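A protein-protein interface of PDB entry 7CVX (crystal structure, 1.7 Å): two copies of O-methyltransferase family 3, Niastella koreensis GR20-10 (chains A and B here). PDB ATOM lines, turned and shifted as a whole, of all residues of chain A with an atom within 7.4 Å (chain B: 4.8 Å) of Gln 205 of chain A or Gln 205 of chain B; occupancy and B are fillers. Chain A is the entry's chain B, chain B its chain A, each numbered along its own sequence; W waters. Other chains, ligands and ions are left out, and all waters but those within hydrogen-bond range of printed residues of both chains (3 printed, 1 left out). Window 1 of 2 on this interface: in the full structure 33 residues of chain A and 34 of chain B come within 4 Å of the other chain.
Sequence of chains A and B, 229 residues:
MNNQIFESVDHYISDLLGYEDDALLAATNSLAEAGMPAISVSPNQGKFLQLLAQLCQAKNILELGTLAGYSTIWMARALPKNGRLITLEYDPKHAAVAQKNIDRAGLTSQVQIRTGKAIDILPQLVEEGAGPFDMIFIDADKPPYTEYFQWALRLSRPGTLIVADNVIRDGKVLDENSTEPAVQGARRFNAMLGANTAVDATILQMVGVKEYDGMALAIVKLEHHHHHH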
ATOM      1  N   ILE A   5      -2.618  -2.854  33.257  1.00  0.00           N
ATOM      2  CA  ILE A   5      -3.598  -3.052  32.157  1.00  0.00           C
ATOM      3  C   ILE A   5      -3.250  -4.344  31.392  1.00  0.00           C
ATOM      4  O   ILE A   5      -4.172  -5.124  31.092  1.00  0.00           O
ATOM      5  CB  ILE A   5      -3.693  -1.828  31.227  1.00  0.00           C
ATOM      6  CG1 ILE A   5      -4.835  -2.002  30.234  1.00  0.00           C
ATOM      7  CG2 ILE A   5      -2.387  -1.537  30.512  1.00  0.00           C
ATOM      8  CD1 ILE A   5      -6.190  -2.113  30.878  1.00  0.00           C
ATOM      9  N   PHE A   6      -1.970  -4.610  31.163  1.00  0.00           N
ATOM     10  CA  PHE A   6      -1.553  -5.787  30.359  1.00  0.00           C
ATOM     11  C   PHE A   6      -1.886  -7.068  31.115  1.00  0.00           C
ATOM     12  O   PHE A   6      -2.338  -8.073  30.510  1.00  0.00           O
ATOM     13  CB  PHE A   6      -0.072  -5.691  30.013  1.00  0.00           C
ATOM     14  CG  PHE A   6       0.295  -4.438  29.282  1.00  0.00           C
ATOM     15  CD1 PHE A   6      -0.315  -4.088  28.096  1.00  0.00           C
ATOM     16  CD2 PHE A   6       1.294  -3.613  29.765  1.00  0.00           C
ATOM     17  CE1 PHE A   6       0.055  -2.948  27.402  1.00  0.00           C
ATOM     18  CE2 PHE A   6       1.675  -2.482  29.071  1.00  0.00           C
ATOM     19  CZ  PHE A   6       1.057  -2.145  27.886  1.00  0.00           C
ATOM     20  N   GLU A   7      -1.706  -7.038  32.430  1.00  0.00           N
ATOM     21  CA  GLU A   7      -2.012  -8.198  33.289  1.00  0.00           C
ATOM     22  C   GLU A   7      -3.522  -8.459  33.240  1.00  0.00           C
ATOM     23  O   GLU A   7      -3.931  -9.582  33.032  1.00  0.00           O
ATOM     24  CB  GLU A   7      -1.527  -7.849  34.682  1.00  0.00           C
ATOM     25  CG  GLU A   7      -1.510  -9.021  35.636  1.00  0.00           C
ATOM     26  CD  GLU A   7      -0.599  -8.748  36.826  1.00  0.00           C
ATOM     27  OE1 GLU A   7      -0.805  -9.393  37.883  1.00  0.00           O
ATOM     28  OE2 GLU A   7       0.294  -7.863  36.697  1.00  0.00           O
ATOM     29  N   SER A   8      -4.334  -7.409  33.366  1.00  0.00           N
ATOM     30  CA  SER A   8      -5.810  -7.527  33.402  1.00  0.00           C
ATOM     31  C   SER A   8      -6.311  -8.061  32.070  1.00  0.00           C
ATOM     32  O   SER A   8      -7.197  -8.911  32.058  1.00  0.00           O
ATOM     33  CB  SER A   8      -6.449  -6.231  33.796  1.00  0.00           C
ATOM     34  OG  SER A   8      -6.031  -5.893  35.101  1.00  0.00           O
ATOM     35  N   VAL A   9      -5.755  -7.558  30.971  1.00  0.00           N
ATOM     36  CA  VAL A   9      -6.132  -8.040  29.620  1.00  0.00           C
ATOM     37  C   VAL A   9      -5.682  -9.498  29.456  1.00  0.00           C
ATOM     38  O   VAL A   9      -6.423 -10.318  28.944  1.00  0.00           O
ATOM     39  CB  VAL A   9      -5.580  -7.092  28.551  1.00  0.00           C
ATOM     40  CG1 VAL A   9      -5.789  -7.689  27.180  1.00  0.00           C
ATOM     41  CG2 VAL A   9      -6.225  -5.714  28.680  1.00  0.00           C
ATOM     42  N   ASP A  10      -4.512  -9.868  29.952  1.00  0.00           N
ATOM     43  CA  ASP A  10      -4.047 -11.270  29.803  1.00  0.00           C
ATOM     44  C   ASP A  10      -5.051 -12.203  30.500  1.00  0.00           C
ATOM     45  O   ASP A  10      -5.353 -13.300  29.944  1.00  0.00           O
ATOM     46  CB  ASP A  10      -2.608 -11.431  30.332  1.00  0.00           C
ATOM     47  CG  ASP A  10      -1.674 -12.370  29.565  1.00  0.00           C
ATOM     48  OD1 ASP A  10      -1.934 -12.647  28.372  1.00  0.00           O
ATOM     49  OD2 ASP A  10      -0.629 -12.756  30.143  1.00  0.00           O
ATOM     50  N   HIS A  11      -5.495 -11.862  31.716  1.00  0.00           N
ATOM     51  CA  HIS A  11      -6.468 -12.687  32.477  1.00  0.00           C
ATOM     52  C   HIS A  11      -7.810 -12.752  31.730  1.00  0.00           C
ATOM     53  O   HIS A  11      -8.406 -13.808  31.682  1.00  0.00           O
ATOM     54  CB  HIS A  11      -6.657 -12.141  33.893  1.00  0.00           C
ATOM     55  CG  HIS A  11      -5.452 -12.229  34.776  1.00  0.00           C
ATOM     56  ND1 HIS A  11      -4.674 -13.375  34.882  1.00  0.00           N
ATOM     57  CD2 HIS A  11      -4.919 -11.346  35.651  1.00  0.00           C
ATOM     58  CE1 HIS A  11      -3.691 -13.174  35.746  1.00  0.00           C
ATOM     59  NE2 HIS A  11      -3.818 -11.939  36.221  1.00  0.00           N
ATOM     60  N   ILE A  13      -8.107 -12.598  28.512  1.00  0.00           N
ATOM     61  CA  ILE A  13      -7.833 -13.509  27.369  1.00  0.00           C
ATOM     62  C   ILE A  13      -7.804 -14.965  27.874  1.00  0.00           C
ATOM     63  O   ILE A  13      -8.414 -15.827  27.213  1.00  0.00           O
ATOM     64  CB  ILE A  13      -6.558 -13.123  26.603  1.00  0.00           C
ATOM     65  CG1 ILE A  13      -6.657 -11.755  25.918  1.00  0.00           C
ATOM     66  CG2 ILE A  13      -6.256 -14.213  25.592  1.00  0.00           C
ATOM     67  CD1 ILE A  13      -5.405 -11.277  25.255  1.00  0.00           C
ATOM     68  N   ASN A  44      -1.237 -18.062  27.929  1.00  0.00           N
ATOM     69  CA  ASN A  44      -1.637 -17.563  26.574  1.00  0.00           C
ATOM     70  C   ASN A  44      -0.478 -17.756  25.575  1.00  0.00           C
ATOM     71  O   ASN A  44      -0.725 -18.125  24.442  1.00  0.00           O
ATOM     72  CB  ASN A  44      -2.101 -16.117  26.613  1.00  0.00           C
ATOM     73  CG  ASN A  44      -3.431 -15.953  27.331  1.00  0.00           C
ATOM     74  OD1 ASN A  44      -4.269 -16.855  27.318  1.00  0.00           O
ATOM     75  ND2 ASN A  44      -3.646 -14.795  27.954  1.00  0.00           N
ATOM     76  N   ILE A 168      13.523  -9.446  23.781  1.00  0.00           N
ATOM     77  CA  ILE A 168      13.285  -7.975  23.908  1.00  0.00           C
ATOM     78  C   ILE A 168      13.696  -7.478  25.309  1.00  0.00           C
ATOM     79  O   ILE A 168      14.175  -6.400  25.412  1.00  0.00           O
ATOM     80  CB  ILE A 168      11.844  -7.611  23.530  1.00  0.00           C
ATOM     81  CG1 ILE A 168      11.620  -7.793  22.025  1.00  0.00           C
ATOM     82  CG2 ILE A 168      11.533  -6.201  23.952  1.00  0.00           C
ATOM     83  CD1 ILE A 168      12.552  -6.972  21.173  1.00  0.00           C
ATOM     84  N   GLY A 171      12.637  -3.968  26.700  1.00  0.00           N
ATOM     85  CA  GLY A 171      13.199  -2.934  25.807  1.00  0.00           C
ATOM     86  C   GLY A 171      14.687  -2.706  26.022  1.00  0.00           C
ATOM     87  O   GLY A 171      15.249  -1.835  25.353  1.00  0.00           O
ATOM     88  N   ILE A 203      10.078 -10.257  14.807  1.00  0.00           N
ATOM     89  CA  ILE A 203      10.015 -10.322  16.287  1.00  0.00           C
ATOM     90  C   ILE A 203       8.652  -9.771  16.725  1.00  0.00           C
ATOM     91  O   ILE A 203       8.271  -8.678  16.234  1.00  0.00           O
ATOM     92  CB  ILE A 203      11.196  -9.540  16.876  1.00  0.00           C
ATOM     93  CG1 ILE A 203      12.530 -10.191  16.514  1.00  0.00           C
ATOM     94  CG2 ILE A 203      10.992  -9.389  18.379  1.00  0.00           C
ATOM     95  CD1 ILE A 203      13.761  -9.350  16.845  1.00  0.00           C
ATOM     96  N   LEU A 204       7.956 -10.504  17.588  1.00  0.00           N
ATOM     97  CA  LEU A 204       6.655 -10.133  18.186  1.00  0.00           C
ATOM     98  C   LEU A 204       6.922  -9.591  19.575  1.00  0.00           C
ATOM     99  O   LEU A 204       7.367 -10.401  20.400  1.00  0.00           O
ATOM    100  CB  LEU A 204       5.741 -11.361  18.294  1.00  0.00           C
ATOM    101  CG  LEU A 204       5.279 -12.006  16.999  1.00  0.00           C
ATOM    102  CD1 LEU A 204       4.461 -13.253  17.323  1.00  0.00           C
ATOM    103  CD2 LEU A 204       4.436 -11.041  16.194  1.00  0.00           C
ATOM    104  N   GLN A 205       6.591  -8.320  19.842  1.00  0.00           N
ATOM    105  CA  GLN A 205       6.584  -7.786  21.240  1.00  0.00           C
ATOM    106  C   GLN A 205       5.425  -8.437  22.009  1.00  0.00           C
ATOM    107  O   GLN A 205       4.359  -8.643  21.431  1.00  0.00           O
ATOM    108  CB  GLN A 205       6.467  -6.259  21.310  1.00  0.00           C
ATOM    109  CG  GLN A 205       7.513  -5.517  20.505  1.00  0.00           C
ATOM    110  CD  GLN A 205       7.482  -4.035  20.783  1.00  0.00           C
ATOM    111  OE1 GLN A 205       7.612  -3.610  21.934  1.00  0.00           O
ATOM    112  NE2 GLN A 205       7.428  -3.254  19.711  1.00  0.00           N
ATOM    113  N   MET A 206       5.664  -8.795  23.264  1.00  0.00           N
ATOM    114  CA  MET A 206       4.732  -9.563  24.103  1.00  0.00           C
ATOM    115  C   MET A 206       4.579  -8.858  25.446  1.00  0.00           C
ATOM    116  O   MET A 206       5.594  -8.523  26.129  1.00  0.00           O
ATOM    117  CB  MET A 206       5.203 -10.998  24.307  1.00  0.00           C
ATOM    118  CG  MET A 206       5.118 -11.754  23.008  1.00  0.00           C
ATOM    119  SD  MET A 206       4.986 -13.484  23.264  1.00  0.00           S
ATOM    120  CE  MET A 206       4.780 -13.987  21.555  1.00  0.00           C
ATOM    121  N   VAL A 207       3.334  -8.586  25.763  1.00  0.00           N
ATOM    122  CA  VAL A 207       2.934  -8.038  27.073  1.00  0.00           C
ATOM    123  C   VAL A 207       1.874  -8.982  27.650  1.00  0.00           C
ATOM    124  O   VAL A 207       1.251  -9.788  26.918  1.00  0.00           O
ATOM    125  CB  VAL A 207       2.449  -6.580  26.915  1.00  0.00           C
ATOM    126  CG1 VAL A 207       3.555  -5.629  26.472  1.00  0.00           C
ATOM    127  CG2 VAL A 207       1.242  -6.454  26.005  1.00  0.00           C
ATOM    128  N   GLY A 208       1.680  -8.902  28.953  1.00  0.00           N
ATOM    129  CA  GLY A 208       0.649  -9.676  29.649  1.00  0.00           C
ATOM    130  C   GLY A 208       1.038  -9.815  31.100  1.00  0.00           C
ATOM    131  O   GLY A 208       1.466  -8.792  31.686  1.00  0.00           O
ATOM    132  N   VAL A 209       0.909 -11.018  31.654  1.00  0.00           N
ATOM    133  CA  VAL A 209       1.176 -11.281  33.100  1.00  0.00           C
ATOM    134  C   VAL A 209       2.684 -11.206  33.368  1.00  0.00           C
ATOM    135  O   VAL A 209       3.027 -10.840  34.510  1.00  0.00           O
ATOM    136  CB  VAL A 209       0.586 -12.622  33.572  1.00  0.00           C
ATOM    137  CG1 VAL A 209      -0.925 -12.569  33.540  1.00  0.00           C
ATOM    138  CG2 VAL A 209       1.074 -13.836  32.797  1.00  0.00           C
ATOM    139  N   TYR A 212       7.364  -7.402  30.187  1.00  0.00           N
ATOM    140  CA  TYR A 212       7.450  -6.982  28.772  1.00  0.00           C
ATOM    141  C   TYR A 212       8.658  -7.663  28.125  1.00  0.00           C
ATOM    142  O   TYR A 212       9.745  -7.554  28.597  1.00  0.00           O
ATOM    143  CB  TYR A 212       7.549  -5.459  28.739  1.00  0.00           C
ATOM    144  CG  TYR A 212       7.932  -4.826  27.428  1.00  0.00           C
ATOM    145  CD1 TYR A 212       7.400  -5.256  26.238  1.00  0.00           C
ATOM    146  CD2 TYR A 212       8.794  -3.752  27.395  1.00  0.00           C
ATOM    147  CE1 TYR A 212       7.747  -4.673  25.037  1.00  0.00           C
ATOM    148  CE2 TYR A 212       9.170  -3.174  26.208  1.00  0.00           C
ATOM    149  CZ  TYR A 212       8.649  -3.628  25.021  1.00  0.00           C
ATOM    150  OH  TYR A 212       8.989  -3.017  23.865  1.00  0.00           O
ATOM    151  N   ASP A 213       8.396  -8.356  27.030  1.00  0.00           N
ATOM    152  CA  ASP A 213       9.447  -9.130  26.331  1.00  0.00           C
ATOM    153  C   ASP A 213       9.028  -9.342  24.862  1.00  0.00           C
ATOM    154  O   ASP A 213       8.291  -8.560  24.352  1.00  0.00           O
ATOM    155  CB  ASP A 213       9.712 -10.413  27.107  1.00  0.00           C
ATOM    156  CG  ASP A 213      11.105 -11.000  26.966  1.00  0.00           C
ATOM    157  OD1 ASP A 213      11.779 -10.639  26.027  1.00  0.00           O
ATOM    158  OD2 ASP A 213      11.441 -11.828  27.776  1.00  0.00           O
ATOM    159  N   GLY A 214       9.574 -10.355  24.208  1.00  0.00           N
ATOM    160  CA  GLY A 214       9.242 -10.614  22.806  1.00  0.00           C
ATOM    161  C   GLY A 214       9.764 -11.967  22.378  1.00  0.00           C
ATOM    162  O   GLY A 214      10.589 -12.504  23.087  1.00  0.00           O
ATOM    163  N   MET A 215       9.223 -12.485  21.283  1.00  0.00           N
ATOM    164  CA  MET A 215       9.634 -13.785  20.736  1.00  0.00           C
ATOM    165  C   MET A 215       9.971 -13.562  19.263  1.00  0.00           C
ATOM    166  O   MET A 215       9.256 -12.865  18.626  1.00  0.00           O
ATOM    167  CB  MET A 215       8.479 -14.788  20.727  1.00  0.00           C
ATOM    168  CG  MET A 215       8.125 -15.320  22.050  1.00  0.00           C
ATOM    169  SD  MET A 215       7.200 -16.889  21.927  1.00  0.00           S
ATOM    170  CE  MET A 215       6.637 -17.065  23.624  1.00  0.00           C
ATOM    171  N   PHE B   6       7.523   1.251  23.334  1.00  0.00           N
ATOM    172  CA  PHE B   6       6.961   0.264  22.378  1.00  0.00           C
ATOM    173  C   PHE B   6       7.266   0.728  20.951  1.00  0.00           C
ATOM    174  O   PHE B   6       7.646  -0.089  20.083  1.00  0.00           O
ATOM    175  CB  PHE B   6       5.463   0.060  22.577  1.00  0.00           C
ATOM    176  CG  PHE B   6       5.104  -0.418  23.953  1.00  0.00           C
ATOM    177  CD1 PHE B   6       5.767  -1.491  24.529  1.00  0.00           C
ATOM    178  CD2 PHE B   6       4.109   0.215  24.671  1.00  0.00           C
ATOM    179  CE1 PHE B   6       5.457  -1.901  25.816  1.00  0.00           C
ATOM    180  CE2 PHE B   6       3.819  -0.189  25.966  1.00  0.00           C
ATOM    181  CZ  PHE B   6       4.481  -1.252  26.533  1.00  0.00           C
ATOM    182  N   VAL B   9      11.130   0.252  20.295  1.00  0.00           N
ATOM    183  CA  VAL B   9      11.392  -1.194  20.056  1.00  0.00           C
ATOM    184  C   VAL B   9      10.839  -1.609  18.677  1.00  0.00           C
ATOM    185  O   VAL B   9      11.524  -2.324  17.920  1.00  0.00           O
ATOM    186  CB  VAL B   9      10.917  -2.075  21.220  1.00  0.00           C
ATOM    187  CG1 VAL B   9      10.946  -3.542  20.863  1.00  0.00           C
ATOM    188  CG2 VAL B   9      11.791  -1.830  22.445  1.00  0.00           C
ATOM    189  N   ASP B  10       9.659  -1.146  18.290  1.00  0.00           N
ATOM    190  CA  ASP B  10       9.095  -1.471  16.951  1.00  0.00           C
ATOM    191  C   ASP B  10      10.050  -0.977  15.869  1.00  0.00           C
ATOM    192  O   ASP B  10      10.275  -1.727  14.901  1.00  0.00           O
ATOM    193  CB  ASP B  10       7.689  -0.900  16.735  1.00  0.00           C
ATOM    194  CG  ASP B  10       6.683  -1.809  16.029  1.00  0.00           C
ATOM    195  OD1 ASP B  10       6.859  -3.033  16.061  1.00  0.00           O
ATOM    196  OD2 ASP B  10       5.647  -1.292  15.623  1.00  0.00           O
ATOM    197  N   ILE B  13      13.024  -3.306  15.627  1.00  0.00           N
ATOM    198  CA  ILE B  13      12.612  -4.558  14.913  1.00  0.00           C
ATOM    199  C   ILE B  13      12.448  -4.322  13.403  1.00  0.00           C
ATOM    200  O   ILE B  13      12.919  -5.169  12.648  1.00  0.00           O
ATOM    201  CB  ILE B  13      11.307  -5.122  15.494  1.00  0.00           C
ATOM    202  CG1 ILE B  13      11.482  -5.478  16.975  1.00  0.00           C
ATOM    203  CG2 ILE B  13      10.820  -6.262  14.632  1.00  0.00           C
ATOM    204  CD1 ILE B  13      10.206  -5.777  17.697  1.00  0.00           C
ATOM    205  N   ILE B 203      -5.724 -14.908  21.598  1.00  0.00           N
ATOM    206  CA  ILE B 203      -5.623 -13.452  21.294  1.00  0.00           C
ATOM    207  C   ILE B 203      -4.209 -13.029  21.667  1.00  0.00           C
ATOM    208  O   ILE B 203      -3.721 -13.387  22.818  1.00  0.00           O
ATOM    209  CB  ILE B 203      -6.681 -12.625  22.028  1.00  0.00           C
ATOM    210  CG1 ILE B 203      -8.089 -12.943  21.536  1.00  0.00           C
ATOM    211  CG2 ILE B 203      -6.379 -11.151  21.910  1.00  0.00           C
ATOM    212  CD1 ILE B 203      -9.182 -12.574  22.529  1.00  0.00           C
ATOM    213  N   LEU B 204      -3.514 -12.401  20.722  1.00  0.00           N
ATOM    214  CA  LEU B 204      -2.163 -11.808  20.953  1.00  0.00           C
ATOM    215  C   LEU B 204      -2.331 -10.314  21.256  1.00  0.00           C
ATOM    216  O   LEU B 204      -2.816  -9.586  20.360  1.00  0.00           O
ATOM    217  CB  LEU B 204      -1.310 -11.972  19.695  1.00  0.00           C
ATOM    218  CG  LEU B 204      -0.886 -13.386  19.333  1.00  0.00           C
ATOM    219  CD1 LEU B 204      -0.345 -13.443  17.888  1.00  0.00           C
ATOM    220  CD2 LEU B 204       0.207 -13.870  20.271  1.00  0.00           C
ATOM    221  N   GLN B 205      -1.895  -9.871  22.426  1.00  0.00           N
ATOM    222  CA  GLN B 205      -1.743  -8.434  22.722  1.00  0.00           C
ATOM    223  C   GLN B 205      -0.661  -7.861  21.804  1.00  0.00           C
ATOM    224  O   GLN B 205       0.387  -8.490  21.617  1.00  0.00           O
ATOM    225  CB  GLN B 205      -1.407  -8.227  24.186  1.00  0.00           C
ATOM    226  CG  GLN B 205      -2.488  -8.694  25.144  1.00  0.00           C
ATOM    227  CD  GLN B 205      -2.421  -8.059  26.523  1.00  0.00           C
ATOM    228  OE1 GLN B 205      -2.488  -6.849  26.704  1.00  0.00           O
ATOM    229  NE2 GLN B 205      -2.316  -8.906  27.520  1.00  0.00           N
ATOM    230  N   MET B 206      -0.905  -6.690  21.240  1.00  0.00           N
ATOM    231  CA  MET B 206       0.075  -6.100  20.312  1.00  0.00           C
ATOM    232  C   MET B 206       0.404  -4.676  20.694  1.00  0.00           C
ATOM    233  O   MET B 206      -0.490  -3.849  20.824  1.00  0.00           O
ATOM    234  CB  MET B 206      -0.453  -6.214  18.889  1.00  0.00           C
ATOM    235  CG  MET B 206      -0.340  -7.661  18.463  1.00  0.00           C
ATOM    236  SD  MET B 206      -0.296  -7.700  16.717  1.00  0.00           S
ATOM    237  CE  MET B 206      -0.140  -9.481  16.513  1.00  0.00           C
ATOM    238  N   VAL B 207       1.696  -4.419  20.828  1.00  0.00           N
ATOM    239  CA  VAL B 207       2.190  -3.038  21.047  1.00  0.00           C
ATOM    240  C   VAL B 207       3.194  -2.689  19.951  1.00  0.00           C
ATOM    241  O   VAL B 207       3.657  -3.572  19.219  1.00  0.00           O
ATOM    242  CB  VAL B 207       2.804  -2.915  22.442  1.00  0.00           C
ATOM    243  CG1 VAL B 207       1.767  -3.086  23.553  1.00  0.00           C
ATOM    244  CG2 VAL B 207       3.949  -3.915  22.600  1.00  0.00           C
ATOM    245  N   GLY B 208       3.505  -1.413  19.801  1.00  0.00           N
ATOM    246  CA  GLY B 208       4.427  -0.966  18.754  1.00  0.00           C
ATOM    247  C   GLY B 208       4.134   0.458  18.377  1.00  0.00           C
ATOM    248  O   GLY B 208       3.789   1.274  19.271  1.00  0.00           O
ATOM    249  N   TYR B 212      -1.928   0.509  21.469  1.00  0.00           N
ATOM    250  CA  TYR B 212      -2.052  -0.815  22.117  1.00  0.00           C
ATOM    251  C   TYR B 212      -3.340  -1.512  21.639  1.00  0.00           C
ATOM    252  O   TYR B 212      -4.407  -0.916  21.661  1.00  0.00           O
ATOM    253  CB  TYR B 212      -2.085  -0.558  23.618  1.00  0.00           C
ATOM    254  CG  TYR B 212      -2.506  -1.703  24.492  1.00  0.00           C
ATOM    255  CD1 TYR B 212      -2.050  -2.977  24.257  1.00  0.00           C
ATOM    256  CD2 TYR B 212      -3.322  -1.496  25.583  1.00  0.00           C
ATOM    257  CE1 TYR B 212      -2.412  -4.033  25.060  1.00  0.00           C
ATOM    258  CE2 TYR B 212      -3.680  -2.540  26.408  1.00  0.00           C
ATOM    259  CZ  TYR B 212      -3.227  -3.810  26.147  1.00  0.00           C
ATOM    260  OH  TYR B 212      -3.561  -4.845  26.934  1.00  0.00           O
ATOM    261  N   ASP B 213      -3.090  -2.808  21.142  1.00  0.00           N
ATOM    262  CA  ASP B 213      -4.251  -3.515  20.557  1.00  0.00           C
ATOM    263  C   ASP B 213      -3.971  -5.019  20.567  1.00  0.00           C
ATOM    264  O   ASP B 213      -3.272  -5.464  21.415  1.00  0.00           O
ATOM    265  CB  ASP B 213      -4.531  -2.990  19.143  1.00  0.00           C
ATOM    266  CG  ASP B 213      -5.982  -3.018  18.694  1.00  0.00           C
ATOM    267  OD1 ASP B 213      -6.705  -3.806  19.226  1.00  0.00           O
ATOM    268  OD2 ASP B 213      -6.312  -2.263  17.769  1.00  0.00           O
ATOM    269  N   GLY B 214      -4.670  -5.716  19.693  1.00  0.00           N
ATOM    270  CA  GLY B 214      -4.448  -7.164  19.673  1.00  0.00           C
ATOM    271  C   GLY B 214      -5.116  -7.801  18.469  1.00  0.00           C
ATOM    272  O   GLY B 214      -5.943  -7.174  17.856  1.00  0.00           O
HETATM  273  O   HOH W   1       1.584  -9.998  23.751  1.00  0.00           O
HETATM  274  O   HOH W   2      -1.672 -15.560  23.197  1.00  0.00           O
HETATM  275  O   HOH W   3       3.188  -6.869  19.614  1.00  0.00           O
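The backbone carbonyl oxygen (O) of Phe 6 of chain B sits at hydrogen-bond distance from the side-chain amide nitrogen (NE2) of Gln 205 of chain A (3.2 Å).
The side-chain amide nitrogen of Gln 205 of chain A lies close to the backbone NH of Asp 10 of chain B.
The side-chain amide nitrogen (NE2) of Gln 205 of chain B lies within hydrogen-bond range of the backbone carbonyl oxygen (O) of Phe 6 of chain A.
The backbone NH of Asp 10 of chain A lies close to the side-chain amide nitrogen of Gln 205 of chain B, at 3.4 Å.
The side-chain carboxylate of Asp 10 of chain A is in hydrogen-bond range of the side-chain amide nitrogen of Asn 44 of chain A, 2.8 Å away.
The backbone NH (N) of Val 209 of chain A is in hydrogen-bond range of the side-chain carboxylate (OD2) of Asp 10 of chain A (2.8 Å).
The side-chain carboxylate of Asp 213 of chain A sits at hydrogen-bond distance from the backbone NH of Ile 168 of chain A (3.1 Å).
OE1 of Gln 205 of chain A sits at hydrogen-bond distance from OH of Tyr 212 of chain A (2.4 Å).
Among the printed residues, merely in contact across the chains: Phe 6 of chain A with Phe 6 of chain B (3.8 Å), Phe 6 of chain A with Tyr 212 of chain B (3.5 Å), Val 9 of chain A with Gln 205 of chain B (3.4 Å), Val 9 of chain A with Tyr 212 of chain B (3.3 Å), Ile 13 of chain A with Ile 203 of chain B (3.5 Å), Ile 13 of chain A with Gln 205 of chain B (3.9 Å), Ile 168 of chain A with Val 9 of chain B (3.8 Å), Gly 171 of chain A with Val 9 of chain B (3.8 Å), Ile 203 of chain A with Ile 13 of chain B (3.8 Å), Gln 205 of chain A with Val 9 of chain B (3.5 Å), Gln 205 of chain A with Ile 13 of chain B (3.9 Å), Gln 205 of chain A with Gln 205 of chain B (3.98 Å), Gln 205 of chain A with Val 207 of chain B (3.7 Å), Gln 205 of chain A with Gly 208 of chain B (3.9 Å), Val 207 of chain A with Gln 205 of chain B (3.7 Å), Gly 208 of chain A with Gln 205 of chain B (3.7 Å), Tyr 212 of chain A with Phe 6 of chain B (3.6 Å) and Tyr 212 of chain A with Val 9 of chain B (3.4 Å).
Gln 205 of chain A touches just these residues of chain B: Phe 6, Val 9, Asp 10, Ile 13, Gln 205, Val 207 and Gly 208.
Gln 205 of chain B touches seven residues of chain A.
Of the printed residues of chain B, Ile 13 of chain A touches Ile 203 (3.5 Å) and Gln 205 (3.9 Å).
Of the printed residues of chain A, Tyr 212 of chain B touches Phe 6 and Val 9.
Val 209 of chain A touches none of the printed residues of chain B.
Asn 44 of chain A touches none of the printed residues of chain B.
The nearest printed residue of chain B that does not touch Gln 205 of chain A is Met 206 of chain B (5.1 Å).
The nearest residue of chain A that does not touch Gln 205 of chain B is Ile 5 of chain A (5.0 Å).
Printed residues of chain B that touch a printed residue of chain A: Phe 6, Val 9, Asp 10, Ile 13, Ile 203, Gln 205, Val 207, Gly 208 and Tyr 212.
Printed residues of chain A that touch a printed residue of chain B: Phe 6, Val 9, Asp 10, Ile 13, Ile 168, Gly 171, Ile 203, Gln 205, Val 207, Gly 208 and Tyr 212.
Hydrophobic or aromatic side chains of chain A within 4 Å of the printed part of chain B: Phe 6, Val 9, Ile 13, Ile 168, Ile 203, Val 207 and Tyr 212.
Among the printed residues, no Asp or Glu carboxylate lies within 4 Å of a Lys or Arg side-chain nitrogen of the other chain.
Phe 6 of chain A touches its own counterpart, Phe 6 of chain B.
Phe 6 of chain A touches Gln 205 of chain B, and with the chains exchanged Gln 205 of chain A touches Phe 6 of chain B.
Phe 6 of chain A touches Tyr 212 of chain B, and with the chains exchanged Tyr 212 of chain A touches Phe 6 of chain B.
Gln 205 of chain A touches its own counterpart, Gln 205 of chain B.
13 positions are printed for both chains.
Of the 22 pairs that touch across the chains among the printed residues, 20 have their exchanged pair printed and touching as well.
Water W3 bridges O of Gln 205 of chain A (2.8 Å) and N of Val 207 of chain B (3.1 Å).
Water W1 lies within hydrogen-bond range of O of Gln 205 of chain B (2.9 Å) and N of Val 207 of chain A (3.0 Å).
Water W2 lies within hydrogen-bond range of O of Asn 44 of chain A (3.0 Å) and O of Ile 203 of chain B (3.0 Å).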
